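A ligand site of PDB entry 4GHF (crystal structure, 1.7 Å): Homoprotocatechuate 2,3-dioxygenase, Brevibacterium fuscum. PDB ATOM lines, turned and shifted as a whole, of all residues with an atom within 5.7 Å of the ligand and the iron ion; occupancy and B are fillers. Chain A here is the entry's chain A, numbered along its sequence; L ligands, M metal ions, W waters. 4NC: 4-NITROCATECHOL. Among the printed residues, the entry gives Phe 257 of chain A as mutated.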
ATOM      1  N   HIS A 155      24.240   2.632 -19.445  1.00  0.00           N
ATOM      2  CA  HIS A 155      24.435   2.599 -20.905  1.00  0.00           C
ATOM      3  C   HIS A 155      24.247   3.916 -21.590  1.00  0.00           C
ATOM      4  O   HIS A 155      23.797   4.909 -20.982  1.00  0.00           O
ATOM      5  CB  HIS A 155      23.467   1.598 -21.500  1.00  0.00           C
ATOM      6  CG  HIS A 155      21.996   1.980 -21.325  1.00  0.00           C
ATOM      7  ND1 HIS A 155      21.228   1.497 -20.313  1.00  0.00           N
ATOM      8  CD2 HIS A 155      21.154   2.717 -22.148  1.00  0.00           C
ATOM      9  CE1 HIS A 155      19.957   1.967 -20.465  1.00  0.00           C
ATOM     10  NE2 HIS A 155      19.918   2.726 -21.570  1.00  0.00           N
ATOM     11  N   ASN A 157      22.669   5.352 -25.529  1.00  0.00           N
ATOM     12  CA  ASN A 157      21.815   4.962 -26.664  1.00  0.00           C
ATOM     13  C   ASN A 157      22.053   5.963 -27.771  1.00  0.00           C
ATOM     14  O   ASN A 157      21.954   7.165 -27.569  1.00  0.00           O
ATOM     15  CB  ASN A 157      20.323   4.929 -26.263  1.00  0.00           C
ATOM     16  CG  ASN A 157      19.433   4.425 -27.349  1.00  0.00           C
ATOM     17  OD1 ASN A 157      19.429   4.952 -28.461  1.00  0.00           O
ATOM     18  ND2 ASN A 157      18.608   3.422 -27.016  1.00  0.00           N
ATOM     19  N   ILE A 181      14.383  -4.796 -32.363  1.00  0.00           N
ATOM     20  CA  ILE A 181      13.029  -4.514 -32.855  1.00  0.00           C
ATOM     21  C   ILE A 181      13.088  -4.547 -34.359  1.00  0.00           C
ATOM     22  O   ILE A 181      13.894  -3.856 -34.979  1.00  0.00           O
ATOM     23  CB  ILE A 181      12.464  -3.159 -32.354  1.00  0.00           C
ATOM     24  CG1 ILE A 181      12.441  -3.128 -30.855  1.00  0.00           C
ATOM     25  CG2 ILE A 181      11.082  -2.883 -32.993  1.00  0.00           C
ATOM     26  CD1 ILE A 181      11.956  -1.798 -30.218  1.00  0.00           C
ATOM     27  N   TRP A 192      20.022  -3.595 -29.093  1.00  0.00           N
ATOM     28  CA  TRP A 192      20.737  -3.389 -27.846  1.00  0.00           C
ATOM     29  C   TRP A 192      21.896  -4.340 -27.773  1.00  0.00           C
ATOM     30  O   TRP A 192      21.758  -5.508 -28.118  1.00  0.00           O
ATOM     31  CB  TRP A 192      19.756  -3.694 -26.745  1.00  0.00           C
ATOM     32  CG  TRP A 192      18.729  -2.614 -26.548  1.00  0.00           C
ATOM     33  CD1 TRP A 192      18.705  -1.650 -25.561  1.00  0.00           C
ATOM     34  CD2 TRP A 192      17.549  -2.371 -27.337  1.00  0.00           C
ATOM     35  NE1 TRP A 192      17.624  -0.829 -25.684  1.00  0.00           N
ATOM     36  CE2 TRP A 192      16.884  -1.195 -26.737  1.00  0.00           C
ATOM     37  CE3 TRP A 192      16.973  -2.993 -28.433  1.00  0.00           C
ATOM     38  CZ2 TRP A 192      15.703  -0.662 -27.247  1.00  0.00           C
ATOM     39  CZ3 TRP A 192      15.789  -2.424 -28.956  1.00  0.00           C
ATOM     40  CH2 TRP A 192      15.157  -1.308 -28.353  1.00  0.00           C
ATOM     41  N   HIS A 200      22.549  -4.023 -22.016  1.00  0.00           N
ATOM     42  CA  HIS A 200      23.344  -3.240 -22.885  1.00  0.00           C
ATOM     43  C   HIS A 200      24.333  -2.303 -22.230  1.00  0.00           C
ATOM     44  O   HIS A 200      24.186  -1.922 -21.074  1.00  0.00           O
ATOM     45  CB  HIS A 200      22.536  -2.465 -23.898  1.00  0.00           C
ATOM     46  CG  HIS A 200      21.450  -1.583 -23.317  1.00  0.00           C
ATOM     47  ND1 HIS A 200      20.668  -1.932 -22.276  1.00  0.00           N
ATOM     48  CD2 HIS A 200      20.997  -0.341 -23.743  1.00  0.00           C
ATOM     49  CE1 HIS A 200      19.742  -0.944 -22.069  1.00  0.00           C
ATOM     50  NE2 HIS A 200      19.954   0.008 -22.980  1.00  0.00           N
ATOM     51  N   HIS A 214      20.256   9.155 -25.379  1.00  0.00           N
ATOM     52  CA  HIS A 214      20.287   9.339 -23.934  1.00  0.00           C
ATOM     53  C   HIS A 214      21.478   8.679 -23.324  1.00  0.00           C
ATOM     54  O   HIS A 214      22.127   7.868 -23.944  1.00  0.00           O
ATOM     55  CB  HIS A 214      18.997   8.855 -23.268  1.00  0.00           C
ATOM     56  CG  HIS A 214      18.663   7.394 -23.491  1.00  0.00           C
ATOM     57  ND1 HIS A 214      17.868   6.973 -24.497  1.00  0.00           N
ATOM     58  CD2 HIS A 214      18.968   6.258 -22.739  1.00  0.00           C
ATOM     59  CE1 HIS A 214      17.706   5.651 -24.433  1.00  0.00           C
ATOM     60  NE2 HIS A 214      18.362   5.200 -23.352  1.00  0.00           N
ATOM     61  N   ALA A 216      22.068   6.596 -19.560  1.00  0.00           N
ATOM     62  CA  ALA A 216      21.213   5.938 -18.580  1.00  0.00           C
ATOM     63  C   ALA A 216      21.955   5.664 -17.279  1.00  0.00           C
ATOM     64  O   ALA A 216      23.105   5.175 -17.318  1.00  0.00           O
ATOM     65  CB  ALA A 216      20.665   4.647 -19.169  1.00  0.00           C
ATOM     66  N   ARG A 243       8.905  10.966 -20.410  1.00  0.00           N
ATOM     67  CA  ARG A 243       8.262   9.686 -20.640  1.00  0.00           C
ATOM     68  C   ARG A 243       8.479   8.810 -19.438  1.00  0.00           C
ATOM     69  O   ARG A 243       9.552   8.755 -18.865  1.00  0.00           O
ATOM     70  CB  ARG A 243       8.816   9.055 -21.927  1.00  0.00           C
ATOM     71  CG  ARG A 243       8.408   7.627 -22.170  1.00  0.00           C
ATOM     72  CD  ARG A 243       8.811   7.037 -23.526  1.00  0.00           C
ATOM     73  NE  ARG A 243       8.558   5.592 -23.395  1.00  0.00           N
ATOM     74  CZ  ARG A 243       9.389   4.613 -23.742  1.00  0.00           C
ATOM     75  NH1 ARG A 243      10.489   4.834 -24.451  1.00  0.00           N
ATOM     76  NH2 ARG A 243       9.060   3.380 -23.480  1.00  0.00           N
ATOM     77  N   HIS A 248       9.828  -1.360 -19.220  1.00  0.00           N
ATOM     78  CA  HIS A 248      10.178  -1.584 -20.629  1.00  0.00           C
ATOM     79  C   HIS A 248       9.799  -3.014 -21.016  1.00  0.00           C
ATOM     80  O   HIS A 248       9.810  -3.947 -20.163  1.00  0.00           O
ATOM     81  CB  HIS A 248      11.676  -1.464 -20.868  1.00  0.00           C
ATOM     82  CG  HIS A 248      12.204  -0.066 -20.941  1.00  0.00           C
ATOM     83  ND1 HIS A 248      11.726   0.869 -21.839  1.00  0.00           N
ATOM     84  CD2 HIS A 248      13.299   0.503 -20.310  1.00  0.00           C
ATOM     85  CE1 HIS A 248      12.475   1.994 -21.706  1.00  0.00           C
ATOM     86  NE2 HIS A 248      13.432   1.760 -20.775  1.00  0.00           N
ATOM     87  N   GLY A 249       9.394  -3.234 -22.262  1.00  0.00           N
ATOM     88  CA  GLY A 249       9.318  -4.574 -22.838  1.00  0.00           C
ATOM     89  C   GLY A 249      10.727  -5.052 -23.083  1.00  0.00           C
ATOM     90  O   GLY A 249      11.211  -5.919 -22.410  1.00  0.00           O
ATOM     91  N   VAL A 250      11.380  -4.472 -24.079  1.00  0.00           N
ATOM     92  CA  VAL A 250      12.779  -4.712 -24.295  1.00  0.00           C
ATOM     93  C   VAL A 250      13.569  -4.341 -23.027  1.00  0.00           C
ATOM     94  O   VAL A 250      13.381  -3.261 -22.447  1.00  0.00           O
ATOM     95  CB  VAL A 250      13.289  -3.774 -25.433  1.00  0.00           C
ATOM     96  CG1 VAL A 250      14.841  -3.836 -25.551  1.00  0.00           C
ATOM     97  CG2 VAL A 250      12.592  -4.103 -26.762  1.00  0.00           C
ATOM     98  N   SER A 251      14.404  -5.248 -22.562  1.00  0.00           N
ATOM     99  CA  SER A 251      15.236  -5.104 -21.333  1.00  0.00           C
ATOM    100  C   SER A 251      14.543  -5.502 -20.031  1.00  0.00           C
ATOM    101  O   SER A 251      15.222  -5.838 -19.076  1.00  0.00           O
ATOM    102  CB  SER A 251      15.896  -3.739 -21.138  1.00  0.00           C
ATOM    103  OG  SER A 251      14.993  -2.773 -20.580  1.00  0.00           O
ATOM    104  N   PHE A 257      12.365   8.660 -18.301  1.00  0.00           N
ATOM    105  CA  PHE A 257      13.124   9.640 -19.164  1.00  0.00           C
ATOM    106  C   PHE A 257      12.826  11.082 -18.752  1.00  0.00           C
ATOM    107  O   PHE A 257      11.651  11.549 -18.772  1.00  0.00           O
ATOM    108  CB  PHE A 257      12.769   9.452 -20.650  1.00  0.00           C
ATOM    109  CG  PHE A 257      13.237   8.129 -21.237  1.00  0.00           C
ATOM    110  CD1 PHE A 257      14.551   7.927 -21.559  1.00  0.00           C
ATOM    111  CD2 PHE A 257      12.388   7.079 -21.329  1.00  0.00           C
ATOM    112  CE1 PHE A 257      15.002   6.686 -22.043  1.00  0.00           C
ATOM    113  CE2 PHE A 257      12.850   5.826 -21.831  1.00  0.00           C
ATOM    114  CZ  PHE A 257      14.135   5.636 -22.151  1.00  0.00           C
ATOM    115  N   GLU A 267      18.088   8.799 -18.924  1.00  0.00           N
ATOM    116  CA  GLU A 267      17.244   7.710 -18.443  1.00  0.00           C
ATOM    117  C   GLU A 267      17.674   7.253 -17.070  1.00  0.00           C
ATOM    118  O   GLU A 267      18.881   7.122 -16.782  1.00  0.00           O
ATOM    119  CB  GLU A 267      17.326   6.517 -19.414  1.00  0.00           C
ATOM    120  CG  GLU A 267      16.288   5.459 -19.144  1.00  0.00           C
ATOM    121  CD  GLU A 267      16.426   4.236 -20.037  1.00  0.00           C
ATOM    122  OE1 GLU A 267      17.449   4.154 -20.716  1.00  0.00           O
ATOM    123  OE2 GLU A 267      15.535   3.338 -20.031  1.00  0.00           O
ATOM    124  N   TYR A 269      17.034   3.882 -14.726  1.00  0.00           N
ATOM    125  CA  TYR A 269      16.820   2.496 -15.168  1.00  0.00           C
ATOM    126  C   TYR A 269      17.079   1.543 -14.011  1.00  0.00           C
ATOM    127  O   TYR A 269      17.966   1.775 -13.180  1.00  0.00           O
ATOM    128  CB  TYR A 269      17.851   2.302 -16.297  1.00  0.00           C
ATOM    129  CG  TYR A 269      17.910   1.042 -17.060  1.00  0.00           C
ATOM    130  CD1 TYR A 269      17.188   0.877 -18.267  1.00  0.00           C
ATOM    131  CD2 TYR A 269      18.793   0.018 -16.679  1.00  0.00           C
ATOM    132  CE1 TYR A 269      17.305  -0.259 -19.040  1.00  0.00           C
ATOM    133  CE2 TYR A 269      18.911  -1.129 -17.461  1.00  0.00           C
ATOM    134  CZ  TYR A 269      18.158  -1.247 -18.641  1.00  0.00           C
ATOM    135  OH  TYR A 269      18.299  -2.378 -19.393  1.00  0.00           O
ATOM    136  N   ARG A 292       6.229  -3.430 -26.514  1.00  0.00           N
ATOM    137  CA  ARG A 292       7.661  -3.625 -26.741  1.00  0.00           C
ATOM    138  C   ARG A 292       8.492  -2.548 -26.062  1.00  0.00           C
ATOM    139  O   ARG A 292       9.618  -2.826 -25.621  1.00  0.00           O
ATOM    140  CB  ARG A 292       7.963  -3.570 -28.251  1.00  0.00           C
ATOM    141  CG  ARG A 292       7.974  -2.215 -28.838  1.00  0.00           C
ATOM    142  CD  ARG A 292       7.898  -2.202 -30.378  1.00  0.00           C
ATOM    143  NE  ARG A 292       7.923  -0.824 -30.783  1.00  0.00           N
ATOM    144  CZ  ARG A 292       6.892   0.018 -30.692  1.00  0.00           C
ATOM    145  NH1 ARG A 292       5.701  -0.403 -30.320  1.00  0.00           N
ATOM    146  NH2 ARG A 292       7.030   1.282 -31.039  1.00  0.00           N
ATOM    147  N   ARG A 293       7.977  -1.347 -25.982  1.00  0.00           N
ATOM    148  CA  ARG A 293       8.751  -0.262 -25.411  1.00  0.00           C
ATOM    149  C   ARG A 293       8.222   0.044 -24.023  1.00  0.00           C
ATOM    150  O   ARG A 293       9.007   0.148 -23.106  1.00  0.00           O
ATOM    151  CB  ARG A 293       8.723   0.960 -26.262  1.00  0.00           C
ATOM    152  CG  ARG A 293       9.652   0.839 -27.476  1.00  0.00           C
ATOM    153  CD  ARG A 293       9.990   2.163 -28.083  1.00  0.00           C
ATOM    154  NE  ARG A 293      10.929   1.961 -29.189  1.00  0.00           N
ATOM    155  CZ  ARG A 293      12.245   1.842 -29.116  1.00  0.00           C
ATOM    156  NH1 ARG A 293      12.900   1.882 -27.963  1.00  0.00           N
ATOM    157  NH2 ARG A 293      12.938   1.737 -30.236  1.00  0.00           N
ATOM    158  N   ASP A 294       6.931   0.285 -23.880  1.00  0.00           N
ATOM    159  CA  ASP A 294       6.305   0.313 -22.574  1.00  0.00           C
ATOM    160  C   ASP A 294       5.465  -0.957 -22.432  1.00  0.00           C
ATOM    161  O   ASP A 294       4.480  -1.120 -23.163  1.00  0.00           O
ATOM    162  CB  ASP A 294       5.440   1.582 -22.354  1.00  0.00           C
ATOM    163  CG  ASP A 294       4.972   1.701 -20.884  1.00  0.00           C
ATOM    164  OD1 ASP A 294       3.809   1.261 -20.582  1.00  0.00           O
ATOM    165  OD2 ASP A 294       5.779   2.196 -20.061  1.00  0.00           O
ATOM    166  N   TRP A 304      10.096  11.601 -28.042  1.00  0.00           N
ATOM    167  CA  TRP A 304      11.037  10.562 -27.733  1.00  0.00           C
ATOM    168  C   TRP A 304      11.661   9.992 -28.998  1.00  0.00           C
ATOM    169  O   TRP A 304      12.850   9.629 -29.027  1.00  0.00           O
ATOM    170  CB  TRP A 304      10.329   9.505 -26.850  1.00  0.00           C
ATOM    171  CG  TRP A 304      11.289   8.571 -26.189  1.00  0.00           C
ATOM    172  CD1 TRP A 304      11.878   8.719 -24.975  1.00  0.00           C
ATOM    173  CD2 TRP A 304      11.869   7.364 -26.767  1.00  0.00           C
ATOM    174  NE1 TRP A 304      12.752   7.689 -24.725  1.00  0.00           N
ATOM    175  CE2 TRP A 304      12.785   6.844 -25.774  1.00  0.00           C
ATOM    176  CE3 TRP A 304      11.697   6.684 -27.947  1.00  0.00           C
ATOM    177  CZ2 TRP A 304      13.549   5.684 -26.003  1.00  0.00           C
ATOM    178  CZ3 TRP A 304      12.450   5.518 -28.157  1.00  0.00           C
ATOM    179  CH2 TRP A 304      13.348   5.028 -27.173  1.00  0.00           C
HETATM  180  C1  4NC L   1      16.191   1.113 -22.755  1.00  0.00           C
HETATM  181  C2  4NC L   1      15.655   2.195 -23.587  1.00  0.00           C
HETATM  182  C3  4NC L   1      14.577   1.954 -24.407  1.00  0.00           C
HETATM  183  C4  4NC L   1      13.986   0.685 -24.393  1.00  0.00           C
HETATM  184  C5  4NC L   1      14.501  -0.350 -23.621  1.00  0.00           C
HETATM  185  C6  4NC L   1      15.618  -0.163 -22.792  1.00  0.00           C
HETATM  186  O7  4NC L   1      17.242   1.325 -21.949  1.00  0.00           O
HETATM  187  O8  4NC L   1      16.170   3.404 -23.561  1.00  0.00           O
HETATM  188  N9  4NC L   1      12.781   0.555 -24.991  1.00  0.00           N
HETATM  189  O10 4NC L   1      11.906   1.829 -25.006  1.00  0.00           O
HETATM  190  O11 4NC L   1      12.053  -0.574 -24.698  1.00  0.00           O
HETATM  191 FE    FE M   1      17.974   3.233 -22.526  1.00  0.00          FE
HETATM  192  O   HOH W   1      18.802   2.137 -24.476  1.00  0.00           O
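O of Arg 292 sits close to O11 of the ligand (3.4 Å).
Merely in contact with the ligand: Trp 192 (3.6 Å), Val 250 (3.3 Å), Ser 251 (3.5 Å), Phe 257 (3.3 Å) and Tyr 269 (3.3 Å).
Hydrophobic or aromatic side chains within 4 Å of the ligand: His 155, Trp 192, His 200, His 214, His 248, Val 250, Phe 257 and Tyr 269.
Of the 19 residues printed, 13 come within 4 Å of the ligand.
Along chain A the residues within 4 Å of the ligand span positions 155 to 293.
An oxygen (O10) of the ligand sits at hydrogen-bond distance from the guanidinium group (NH1) of Arg 293 (3.1 Å).
An oxygen (O10) of the ligand is in hydrogen-bond range of the guanidinium group (NH1) of Arg 243.
ND1 of His 248 sits at hydrogen-bond distance from O11 of the ligand.
A ring nitrogen (NE2) of His 200 lies close to an oxygen (O7) of the ligand, at 3.2 Å.
A ring nitrogen (NE2) of His 200 sits close to a ring nitrogen (ND1) of His 155 (3.3 Å).
The side-chain carboxylate (OE2) of Glu 267 is in hydrogen-bond range of a ring nitrogen (NE2) of His 248 (2.7 Å).
O of His 155 is in hydrogen-bond range of N of Ala 216 (2.8 Å).
The backbone carbonyl oxygen (O) of Arg 293 sits at hydrogen-bond distance from a ring nitrogen (ND1) of His 248 (3.1 Å).
The backbone carbonyl oxygen of Arg 293 sits at hydrogen-bond distance from the guanidinium group of Arg 243, at 3.3 Å.
N of Phe 257 is in hydrogen-bond range of O of Arg 243, at 2.9 Å.
The backbone carbonyl oxygen of Arg 292 lies close to the backbone NH of Gly 249, at 3.4 Å.
The backbone NH (N) of Asn 157 is in hydrogen-bond range of the backbone carbonyl oxygen (O) of His 214 (3.0 Å).
Water W1 lies within hydrogen-bond range of NE2 of His 200 (2.8 Å), ND2 of Asn 157 (2.9 Å) and NE1 of Trp 192 (3.4 Å).
His 200 touches the iron ion.
Within 4 Å of the iron ion: His 155, His 200, His 214 and Glu 267.
The nearest printed residue that does not touch the iron ion is Ala 216 (4.5 Å).
The iron ion is bound by O8 of the ligand (2.1 Å), OE1 of Glu 267 (2.1 Å), O7 of the ligand (2.1 Å), NE2 of His 214 (2.2 Å), NE2 of His 155 (2.2 Å) and water W1 (2.4 Å).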
